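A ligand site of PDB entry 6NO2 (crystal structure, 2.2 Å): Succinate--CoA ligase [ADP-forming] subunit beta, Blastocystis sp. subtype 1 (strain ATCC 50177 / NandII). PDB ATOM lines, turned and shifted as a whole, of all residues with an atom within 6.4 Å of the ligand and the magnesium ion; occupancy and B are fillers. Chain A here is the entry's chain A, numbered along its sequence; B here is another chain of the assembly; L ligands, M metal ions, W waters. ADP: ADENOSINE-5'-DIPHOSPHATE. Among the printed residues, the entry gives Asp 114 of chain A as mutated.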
ATOM      1  N   GLU A   5      -6.431  16.436  -0.460  1.00  0.00           N
ATOM      2  CA  GLU A   5      -7.309  15.754  -1.410  1.00  0.00           C
ATOM      3  C   GLU A   5      -6.503  14.937  -2.418  1.00  0.00           C
ATOM      4  O   GLU A   5      -6.730  13.730  -2.581  1.00  0.00           O
ATOM      5  CB  GLU A   5      -8.184  16.788  -2.122  1.00  0.00           C
ATOM      6  CG  GLU A   5      -9.352  16.208  -2.895  1.00  0.00           C
ATOM      7  CD  GLU A   5     -10.129  17.279  -3.649  1.00  0.00           C
ATOM      8  OE1 GLU A   5      -9.969  18.471  -3.329  1.00  0.00           O
ATOM      9  OE2 GLU A   5     -10.910  16.931  -4.566  1.00  0.00           O
ATOM     10  N   LYS A   9      -6.634  10.785  -2.753  1.00  0.00           N
ATOM     11  CA  LYS A   9      -7.164  10.173  -3.969  1.00  0.00           C
ATOM     12  C   LYS A   9      -6.151   9.242  -4.615  1.00  0.00           C
ATOM     13  O   LYS A   9      -6.475   8.109  -4.986  1.00  0.00           O
ATOM     14  CB  LYS A   9      -7.612  11.260  -4.945  1.00  0.00           C
ATOM     15  CG  LYS A   9      -8.907  11.944  -4.539  1.00  0.00           C
ATOM     16  CD  LYS A   9      -9.256  13.080  -5.491  1.00  0.00           C
ATOM     17  CE  LYS A   9     -10.623  13.669  -5.172  1.00  0.00           C
ATOM     18  NZ  LYS A   9     -10.928  14.845  -6.011  1.00  0.00           N
ATOM     19  N   GLN A  20     -11.203  10.849  -8.880  1.00  0.00           N
ATOM     20  CA  GLN A  20     -10.788  11.874  -9.837  1.00  0.00           C
ATOM     21  C   GLN A  20      -9.775  12.777  -9.141  1.00  0.00           C
ATOM     22  O   GLN A  20     -10.124  13.769  -8.504  1.00  0.00           O
ATOM     23  CB  GLN A  20     -11.995  12.659 -10.349  1.00  0.00           C
ATOM     24  CG  GLN A  20     -11.628  13.675 -11.411  1.00  0.00           C
ATOM     25  CD  GLN A  20     -12.813  14.498 -11.880  1.00  0.00           C
ATOM     26  OE1 GLN A  20     -13.636  14.933 -11.076  1.00  0.00           O
ATOM     27  NE2 GLN A  20     -12.905  14.714 -13.185  1.00  0.00           N
ATOM     28  N   VAL A  48     -13.150  21.652 -14.321  1.00  0.00           N
ATOM     29  CA  VAL A  48     -13.471  22.077 -12.963  1.00  0.00           C
ATOM     30  C   VAL A  48     -12.172  22.493 -12.297  1.00  0.00           C
ATOM     31  O   VAL A  48     -11.159  21.791 -12.395  1.00  0.00           O
ATOM     32  CB  VAL A  48     -14.178  20.971 -12.161  1.00  0.00           C
ATOM     33  CG1 VAL A  48     -14.445  21.440 -10.740  1.00  0.00           C
ATOM     34  CG2 VAL A  48     -15.467  20.562 -12.848  1.00  0.00           C
ATOM     35  N   LYS A  50     -10.617  23.455  -8.601  1.00  0.00           N
ATOM     36  CA  LYS A  50     -10.909  23.273  -7.187  1.00  0.00           C
ATOM     37  C   LYS A  50      -9.761  23.851  -6.353  1.00  0.00           C
ATOM     38  O   LYS A  50      -8.622  23.387  -6.469  1.00  0.00           O
ATOM     39  CB  LYS A  50     -11.099  21.787  -6.849  1.00  0.00           C
ATOM     40  CG  LYS A  50     -12.149  21.087  -7.692  1.00  0.00           C
ATOM     41  CD  LYS A  50     -12.205  19.593  -7.393  1.00  0.00           C
ATOM     42  CE  LYS A  50     -12.567  19.315  -5.936  1.00  0.00           C
ATOM     43  NZ  LYS A  50     -12.769  17.869  -5.668  1.00  0.00           N
ATOM     44  N   ALA A  55      -9.234  23.163   4.392  1.00  0.00           N
ATOM     45  CA  ALA A  55     -10.466  23.682   4.944  1.00  0.00           C
ATOM     46  C   ALA A  55     -11.631  23.119   4.149  1.00  0.00           C
ATOM     47  O   ALA A  55     -11.518  22.937   2.937  1.00  0.00           O
ATOM     48  CB  ALA A  55     -10.495  25.216   4.921  1.00  0.00           C
ATOM     49  N   GLY A  56     -12.747  22.852   4.829  1.00  0.00           N
ATOM     50  CA  GLY A  56     -13.896  22.249   4.187  1.00  0.00           C
ATOM     51  C   GLY A  56     -14.918  23.275   3.722  1.00  0.00           C
ATOM     52  O   GLY A  56     -14.851  24.458   4.035  1.00  0.00           O
ATOM     53  N   GLY A  57     -15.895  22.787   2.955  1.00  0.00           N
ATOM     54  CA  GLY A  57     -16.951  23.643   2.444  1.00  0.00           C
ATOM     55  C   GLY A  57     -16.513  24.597   1.355  1.00  0.00           C
ATOM     56  O   GLY A  57     -16.972  25.749   1.317  1.00  0.00           O
ATOM     57  N   ARG A  58     -15.621  24.156   0.470  1.00  0.00           N
ATOM     58  CA  ARG A  58     -15.140  25.028  -0.600  1.00  0.00           C
ATOM     59  C   ARG A  58     -16.272  25.389  -1.556  1.00  0.00           C
ATOM     60  O   ARG A  58     -16.347  26.522  -2.046  1.00  0.00           O
ATOM     61  CB  ARG A  58     -14.011  24.339  -1.354  1.00  0.00           C
ATOM     62  CG  ARG A  58     -12.832  23.937  -0.492  1.00  0.00           C
ATOM     63  CD  ARG A  58     -11.839  23.089  -1.265  1.00  0.00           C
ATOM     64  NE  ARG A  58     -12.412  21.808  -1.676  1.00  0.00           N
ATOM     65  CZ  ARG A  58     -11.760  20.875  -2.371  1.00  0.00           C
ATOM     66  NH1 ARG A  58     -10.505  21.080  -2.745  1.00  0.00           N
ATOM     67  NH2 ARG A  58     -12.366  19.745  -2.687  1.00  0.00           N
ATOM     68  N   GLY A  59     -17.160  24.428  -1.842  1.00  0.00           N
ATOM     69  CA  GLY A  59     -18.202  24.660  -2.834  1.00  0.00           C
ATOM     70  C   GLY A  59     -19.067  25.861  -2.529  1.00  0.00           C
ATOM     71  O   GLY A  59     -19.574  26.514  -3.451  1.00  0.00           O
ATOM     72  N   LYS A  60     -19.256  26.177  -1.249  1.00  0.00           N
ATOM     73  CA  LYS A  60     -20.131  27.270  -0.832  1.00  0.00           C
ATOM     74  C   LYS A  60     -19.375  28.444  -0.222  1.00  0.00           C
ATOM     75  O   LYS A  60     -19.994  29.309   0.391  1.00  0.00           O
ATOM     76  CB  LYS A  60     -21.167  26.754   0.166  1.00  0.00           C
ATOM     77  CG  LYS A  60     -22.124  25.732  -0.411  1.00  0.00           C
ATOM     78  CD  LYS A  60     -23.343  25.532   0.473  1.00  0.00           C
ATOM     79  CE  LYS A  60     -24.350  24.584  -0.149  1.00  0.00           C
ATOM     80  NZ  LYS A  60     -25.616  24.521   0.632  1.00  0.00           N
ATOM     81  N   VAL A  71     -15.069  25.774  -5.968  1.00  0.00           N
ATOM     82  CA  VAL A  71     -15.154  24.773  -7.030  1.00  0.00           C
ATOM     83  C   VAL A  71     -15.970  25.392  -8.154  1.00  0.00           C
ATOM     84  O   VAL A  71     -17.160  25.680  -7.970  1.00  0.00           O
ATOM     85  CB  VAL A  71     -15.796  23.458  -6.548  1.00  0.00           C
ATOM     86  CG1 VAL A  71     -15.899  22.447  -7.686  1.00  0.00           C
ATOM     87  CG2 VAL A  71     -15.001  22.879  -5.384  1.00  0.00           C
ATOM     88  N   LEU A  73     -16.763  25.848 -12.575  1.00  0.00           N
ATOM     89  CA  LEU A  73     -16.762  25.269 -13.912  1.00  0.00           C
ATOM     90  C   LEU A  73     -16.077  26.222 -14.892  1.00  0.00           C
ATOM     91  O   LEU A  73     -16.202  27.442 -14.792  1.00  0.00           O
ATOM     92  CB  LEU A  73     -18.189  24.982 -14.361  1.00  0.00           C
ATOM     93  CG  LEU A  73     -18.406  24.291 -15.705  1.00  0.00           C
ATOM     94  CD1 LEU A  73     -17.962  22.834 -15.657  1.00  0.00           C
ATOM     95  CD2 LEU A  73     -19.870  24.397 -16.113  1.00  0.00           C
ATOM     96  N   CYS A 110      -9.660  19.560 -12.976  1.00  0.00           N
ATOM     97  CA  CYS A 110     -10.291  18.294 -13.297  1.00  0.00           C
ATOM     98  C   CYS A 110     -11.159  18.439 -14.540  1.00  0.00           C
ATOM     99  O   CYS A 110     -11.670  19.527 -14.843  1.00  0.00           O
ATOM    100  CB  CYS A 110     -11.169  17.783 -12.149  1.00  0.00           C
ATOM    101  SG  CYS A 110     -10.368  17.778 -10.534  1.00  0.00           S
ATOM    102  N   GLY A 111     -11.325  17.334 -15.261  1.00  0.00           N
ATOM    103  CA  GLY A 111     -12.311  17.293 -16.320  1.00  0.00           C
ATOM    104  C   GLY A 111     -13.714  17.273 -15.741  1.00  0.00           C
ATOM    105  O   GLY A 111     -13.990  16.624 -14.739  1.00  0.00           O
ATOM    106  N   ALA A 112     -14.613  18.027 -16.377  1.00  0.00           N
ATOM    107  CA  ALA A 112     -15.998  18.056 -15.949  1.00  0.00           C
ATOM    108  C   ALA A 112     -16.696  16.777 -16.391  1.00  0.00           C
ATOM    109  O   ALA A 112     -16.526  16.312 -17.530  1.00  0.00           O
ATOM    110  CB  ALA A 112     -16.720  19.269 -16.531  1.00  0.00           C
ATOM    111  N   VAL A 113     -17.476  16.191 -15.491  1.00  0.00           N
ATOM    112  CA  VAL A 113     -18.190  14.946 -15.738  1.00  0.00           C
ATOM    113  C   VAL A 113     -19.637  15.107 -15.298  1.00  0.00           C
ATOM    114  O   VAL A 113     -19.962  15.935 -14.435  1.00  0.00           O
ATOM    115  CB  VAL A 113     -17.540  13.740 -15.028  1.00  0.00           C
ATOM    116  CG1 VAL A 113     -16.169  13.433 -15.609  1.00  0.00           C
ATOM    117  CG2 VAL A 113     -17.441  14.004 -13.529  1.00  0.00           C
ATOM    118  N   ASP A 114     -20.510  14.308 -15.891  1.00  0.00           N
ATOM    119  CA  ASP A 114     -21.890  14.217 -15.443  1.00  0.00           C
ATOM    120  C   ASP A 114     -21.915  13.486 -14.103  1.00  0.00           C
ATOM    121  O   ASP A 114     -21.469  12.337 -14.008  1.00  0.00           O
ATOM    122  CB  ASP A 114     -22.745  13.486 -16.469  1.00  0.00           C
ATOM    123  CG  ASP A 114     -22.843  14.231 -17.791  1.00  0.00           C
ATOM    124  OD1 ASP A 114     -22.806  15.479 -17.780  1.00  0.00           O
ATOM    125  OD2 ASP A 114     -22.943  13.558 -18.838  1.00  0.00           O
ATOM    126  N   ILE A 115     -22.436  14.148 -13.075  1.00  0.00           N
ATOM    127  CA  ILE A 115     -22.597  13.552 -11.756  1.00  0.00           C
ATOM    128  C   ILE A 115     -24.067  13.199 -11.587  1.00  0.00           C
ATOM    129  O   ILE A 115     -24.930  14.091 -11.553  1.00  0.00           O
ATOM    130  CB  ILE A 115     -22.123  14.497 -10.644  1.00  0.00           C
ATOM    131  CG1 ILE A 115     -20.630  14.797 -10.820  1.00  0.00           C
ATOM    132  CG2 ILE A 115     -22.387  13.880  -9.271  1.00  0.00           C
ATOM    133  CD1 ILE A 115     -20.100  15.870  -9.910  1.00  0.00           C
ATOM    134  N   GLU A 118     -24.787  11.686  -5.551  1.00  0.00           N
ATOM    135  CA  GLU A 118     -23.737  12.028  -4.593  1.00  0.00           C
ATOM    136  C   GLU A 118     -24.075  11.414  -3.252  1.00  0.00           C
ATOM    137  O   GLU A 118     -25.153  11.685  -2.698  1.00  0.00           O
ATOM    138  CB  GLU A 118     -23.569  13.543  -4.472  1.00  0.00           C
ATOM    139  CG  GLU A 118     -22.917  14.200  -5.669  1.00  0.00           C
ATOM    140  CD  GLU A 118     -22.599  15.667  -5.434  1.00  0.00           C
ATOM    141  OE1 GLU A 118     -22.980  16.188  -4.362  1.00  0.00           O
ATOM    142  OE2 GLU A 118     -21.974  16.295  -6.314  1.00  0.00           O
ATOM    143  N   ASN A 210     -16.510  12.676   0.567  1.00  0.00           N
ATOM    144  CA  ASN A 210     -17.653  13.594   0.564  1.00  0.00           C
ATOM    145  C   ASN A 210     -17.522  14.549  -0.621  1.00  0.00           C
ATOM    146  O   ASN A 210     -16.869  15.596  -0.511  1.00  0.00           O
ATOM    147  CB  ASN A 210     -17.737  14.374   1.868  1.00  0.00           C
ATOM    148  CG  ASN A 210     -18.979  15.247   1.948  1.00  0.00           C
ATOM    149  OD1 ASN A 210     -19.980  14.971   1.301  1.00  0.00           O
ATOM    150  ND2 ASN A 210     -18.902  16.315   2.731  1.00  0.00           N
ATOM    151  N   PRO A 211     -18.156  14.237  -1.771  1.00  0.00           N
ATOM    152  CA  PRO A 211     -19.064  13.127  -2.045  1.00  0.00           C
ATOM    153  C   PRO A 211     -18.422  11.919  -2.732  1.00  0.00           C
ATOM    154  O   PRO A 211     -17.519  12.069  -3.542  1.00  0.00           O
ATOM    155  CB  PRO A 211     -20.088  13.758  -2.984  1.00  0.00           C
ATOM    156  CG  PRO A 211     -19.271  14.707  -3.796  1.00  0.00           C
ATOM    157  CD  PRO A 211     -18.157  15.201  -2.888  1.00  0.00           C
ATOM    158  N   LEU A 227     -15.090  11.787  -5.582  1.00  0.00           N
ATOM    159  CA  LEU A 227     -14.915  13.156  -6.058  1.00  0.00           C
ATOM    160  C   LEU A 227     -14.268  14.059  -5.010  1.00  0.00           C
ATOM    161  O   LEU A 227     -13.898  15.194  -5.339  1.00  0.00           O
ATOM    162  CB  LEU A 227     -16.261  13.751  -6.486  1.00  0.00           C
ATOM    163  CG  LEU A 227     -16.993  12.941  -7.565  1.00  0.00           C
ATOM    164  CD1 LEU A 227     -18.405  13.454  -7.772  1.00  0.00           C
ATOM    165  CD2 LEU A 227     -16.217  12.982  -8.872  1.00  0.00           C
ATOM    166  N   ASP A 228     -14.135  13.585  -3.780  1.00  0.00           N
ATOM    167  CA  ASP A 228     -13.402  14.260  -2.730  1.00  0.00           C
ATOM    168  C   ASP A 228     -12.880  13.202  -1.778  1.00  0.00           C
ATOM    169  O   ASP A 228     -13.444  12.101  -1.692  1.00  0.00           O
ATOM    170  CB  ASP A 228     -14.272  15.297  -1.999  1.00  0.00           C
ATOM    171  CG  ASP A 228     -13.457  16.353  -1.287  1.00  0.00           C
ATOM    172  OD1 ASP A 228     -12.208  16.255  -1.276  1.00  0.00           O
ATOM    173  OD2 ASP A 228     -14.065  17.302  -0.742  1.00  0.00           O
ATOM    174  N   ALA A 229     -11.812  13.525  -1.066  1.00  0.00           N
ATOM    175  CA  ALA A 229     -11.185  12.552  -0.179  1.00  0.00           C
ATOM    176  C   ALA A 229     -10.442  13.274   0.930  1.00  0.00           C
ATOM    177  O   ALA A 229      -9.809  14.304   0.697  1.00  0.00           O
ATOM    178  CB  ALA A 229     -10.229  11.633  -0.942  1.00  0.00           C
ATOM    179  N   GLN B  41      -8.268  12.093 -14.762  1.00  0.00           N
ATOM    180  CA  GLN B  41      -9.113  13.182 -15.239  1.00  0.00           C
ATOM    181  C   GLN B  41     -10.535  12.721 -15.538  1.00  0.00           C
ATOM    182  O   GLN B  41     -11.507  13.358 -15.117  1.00  0.00           O
ATOM    183  CB  GLN B  41      -8.482  13.810 -16.490  1.00  0.00           C
ATOM    184  CG  GLN B  41      -7.175  14.538 -16.220  1.00  0.00           C
ATOM    185  CD  GLN B  41      -7.379  15.819 -15.444  1.00  0.00           C
ATOM    186  OE1 GLN B  41      -8.480  16.118 -14.998  1.00  0.00           O
ATOM    187  NE2 GLN B  41      -6.309  16.590 -15.281  1.00  0.00           N
HETATM  188  PB  ADP L   1     -16.530  20.696  -0.968  1.00  0.00           P
HETATM  189  O1B ADP L   1     -15.498  21.124   0.024  1.00  0.00           O
HETATM  190  O2B ADP L   1     -17.544  21.792  -1.271  1.00  0.00           O
HETATM  191  O3B ADP L   1     -17.295  19.445  -0.529  1.00  0.00           O
HETATM  192  PA  ADP L   1     -15.892  19.023  -3.278  1.00  0.00           P
HETATM  193  O1A ADP L   1     -14.537  18.582  -3.668  1.00  0.00           O
HETATM  194  O2A ADP L   1     -16.720  17.983  -2.536  1.00  0.00           O
HETATM  195  O3A ADP L   1     -15.852  20.328  -2.362  1.00  0.00           O
HETATM  196  O5' ADP L   1     -16.752  19.456  -4.564  1.00  0.00           O
HETATM  197  C5' ADP L   1     -17.878  20.351  -4.565  1.00  0.00           C
HETATM  198  C4' ADP L   1     -18.807  19.967  -5.686  1.00  0.00           C
HETATM  199  O4' ADP L   1     -18.130  20.078  -6.953  1.00  0.00           O
HETATM  200  C3' ADP L   1     -19.307  18.528  -5.666  1.00  0.00           C
HETATM  201  O3' ADP L   1     -20.422  18.398  -4.796  1.00  0.00           O
HETATM  202  C2' ADP L   1     -19.695  18.287  -7.120  1.00  0.00           C
HETATM  203  O2' ADP L   1     -21.061  18.602  -7.359  1.00  0.00           O
HETATM  204  C1' ADP L   1     -18.778  19.251  -7.899  1.00  0.00           C
HETATM  205  N9  ADP L   1     -17.751  18.579  -8.695  1.00  0.00           N
HETATM  206  C8  ADP L   1     -16.560  18.054  -8.263  1.00  0.00           C
HETATM  207  N7  ADP L   1     -15.845  17.501  -9.205  1.00  0.00           N
HETATM  208  C5  ADP L   1     -16.615  17.673 -10.349  1.00  0.00           C
HETATM  209  C6  ADP L   1     -16.420  17.287 -11.688  1.00  0.00           C
HETATM  210  N6  ADP L   1     -15.335  16.646 -12.127  1.00  0.00           N
HETATM  211  N1  ADP L   1     -17.392  17.605 -12.581  1.00  0.00           N
HETATM  212  C2  ADP L   1     -18.470  18.252 -12.146  1.00  0.00           C
HETATM  213  N3  ADP L   1     -18.763  18.663 -10.907  1.00  0.00           N
HETATM  214  C4  ADP L   1     -17.790  18.336 -10.050  1.00  0.00           C
HETATM  215 MG    MG M   1     -16.000  17.782  -0.045  1.00  0.00          MG
HETATM  216  O   HOH W   1     -13.359  16.103  -8.316  1.00  0.00           O
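The side-chain amide nitrogen of Gln 20 is in hydrogen-bond range of the backbone carbonyl oxygen of Gly 111, at 2.7 Å.
The backbone carbonyl oxygen (O) of Gln 20 is in hydrogen-bond range of the side-chain amino group (NZ) of Lys 9.
The side-chain amide nitrogen (NE2) of Gln 20 is in hydrogen-bond range of the backbone carbonyl oxygen (O) of Gln 41 of chain B.
The guanidinium group of Arg 58 lies within salt-bridge range of the side-chain carboxylate of Glu 5 (2.7 Å).
The side-chain amino group (NZ) of Lys 50 sits at hydrogen-bond distance from the backbone carbonyl oxygen (O) of Leu 227, at 2.9 Å.
The side-chain amino group (NZ) of Lys 50 is in salt-bridge range of the side-chain carboxylate (OE1) of Glu 5 (3.7 Å).
The backbone NH (N) of Gly 111 sits at hydrogen-bond distance from the side-chain amide oxygen (OE1) of Gln 41 of chain B (3.1 Å).
The backbone carbonyl oxygen (O) of Leu 227 is in hydrogen-bond range of the side-chain amino group (NZ) of Lys 9 (3.1 Å).
Residues that only touch the ligand: Pro 211 (3.2 Å), Ile 115 (3.3 Å), Val 71 (3.3 Å), Val 48 (3.5 Å), Ala 112 (3.7 Å) and Leu 227 (3.8 Å).
Hydrophobic or aromatic side chains within 4 Å of the ligand: Val 48, Val 71, Val 113, Ile 115 and Pro 211.
Within 4 Å of the ligand: Gln 20, Val 48, Lys 50, Gly 57, Arg 58, Gly 59, Val 71, Gly 111, Ala 112, Val 113, Ile 115, Glu 118, Asn 210, Pro 211, Leu 227 and Asp 228.
The side-chain amide oxygen (OE1) of Gln 20 is in hydrogen-bond range of a nitrogen (N6) of the ligand (2.6 Å).
The backbone NH (N) of Arg 58 sits at hydrogen-bond distance from an oxygen (O1B) of the ligand (3.1 Å).
The guanidinium group of Arg 58 is in salt-bridge range of an oxygen (O1A) of the ligand, 2.7 Å away.
An oxygen (O2') of the ligand is in hydrogen-bond range of the side-chain carboxylate of Glu 118 (2.7 Å).
An oxygen (O2B) of the ligand sits at hydrogen-bond distance from the backbone NH of Gly 59 (2.7 Å).
An oxygen (O1A) of the ligand lies within salt-bridge range of the side-chain amino group (NZ) of Lys 50 (2.8 Å).
A nitrogen (N6) of the ligand is in hydrogen-bond range of the backbone carbonyl oxygen of Gly 111, 2.9 Å away.
A nitrogen (N1) of the ligand sits at hydrogen-bond distance from the backbone NH (N) of Val 113.
The backbone NH (N) of Gly 57 is in hydrogen-bond range of an oxygen (O1B) of the ligand.
The magnesium ion is bound by OD2 of Asp 228 (2.1 Å), O3B of the ligand (2.2 Å) and O of Asn 210 (2.4 Å).
The magnesium ion has three donor atoms within binding distance.
Slightly farther from the magnesium ion lies an oxygen (O2A) of the ligand (2.6 Å).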
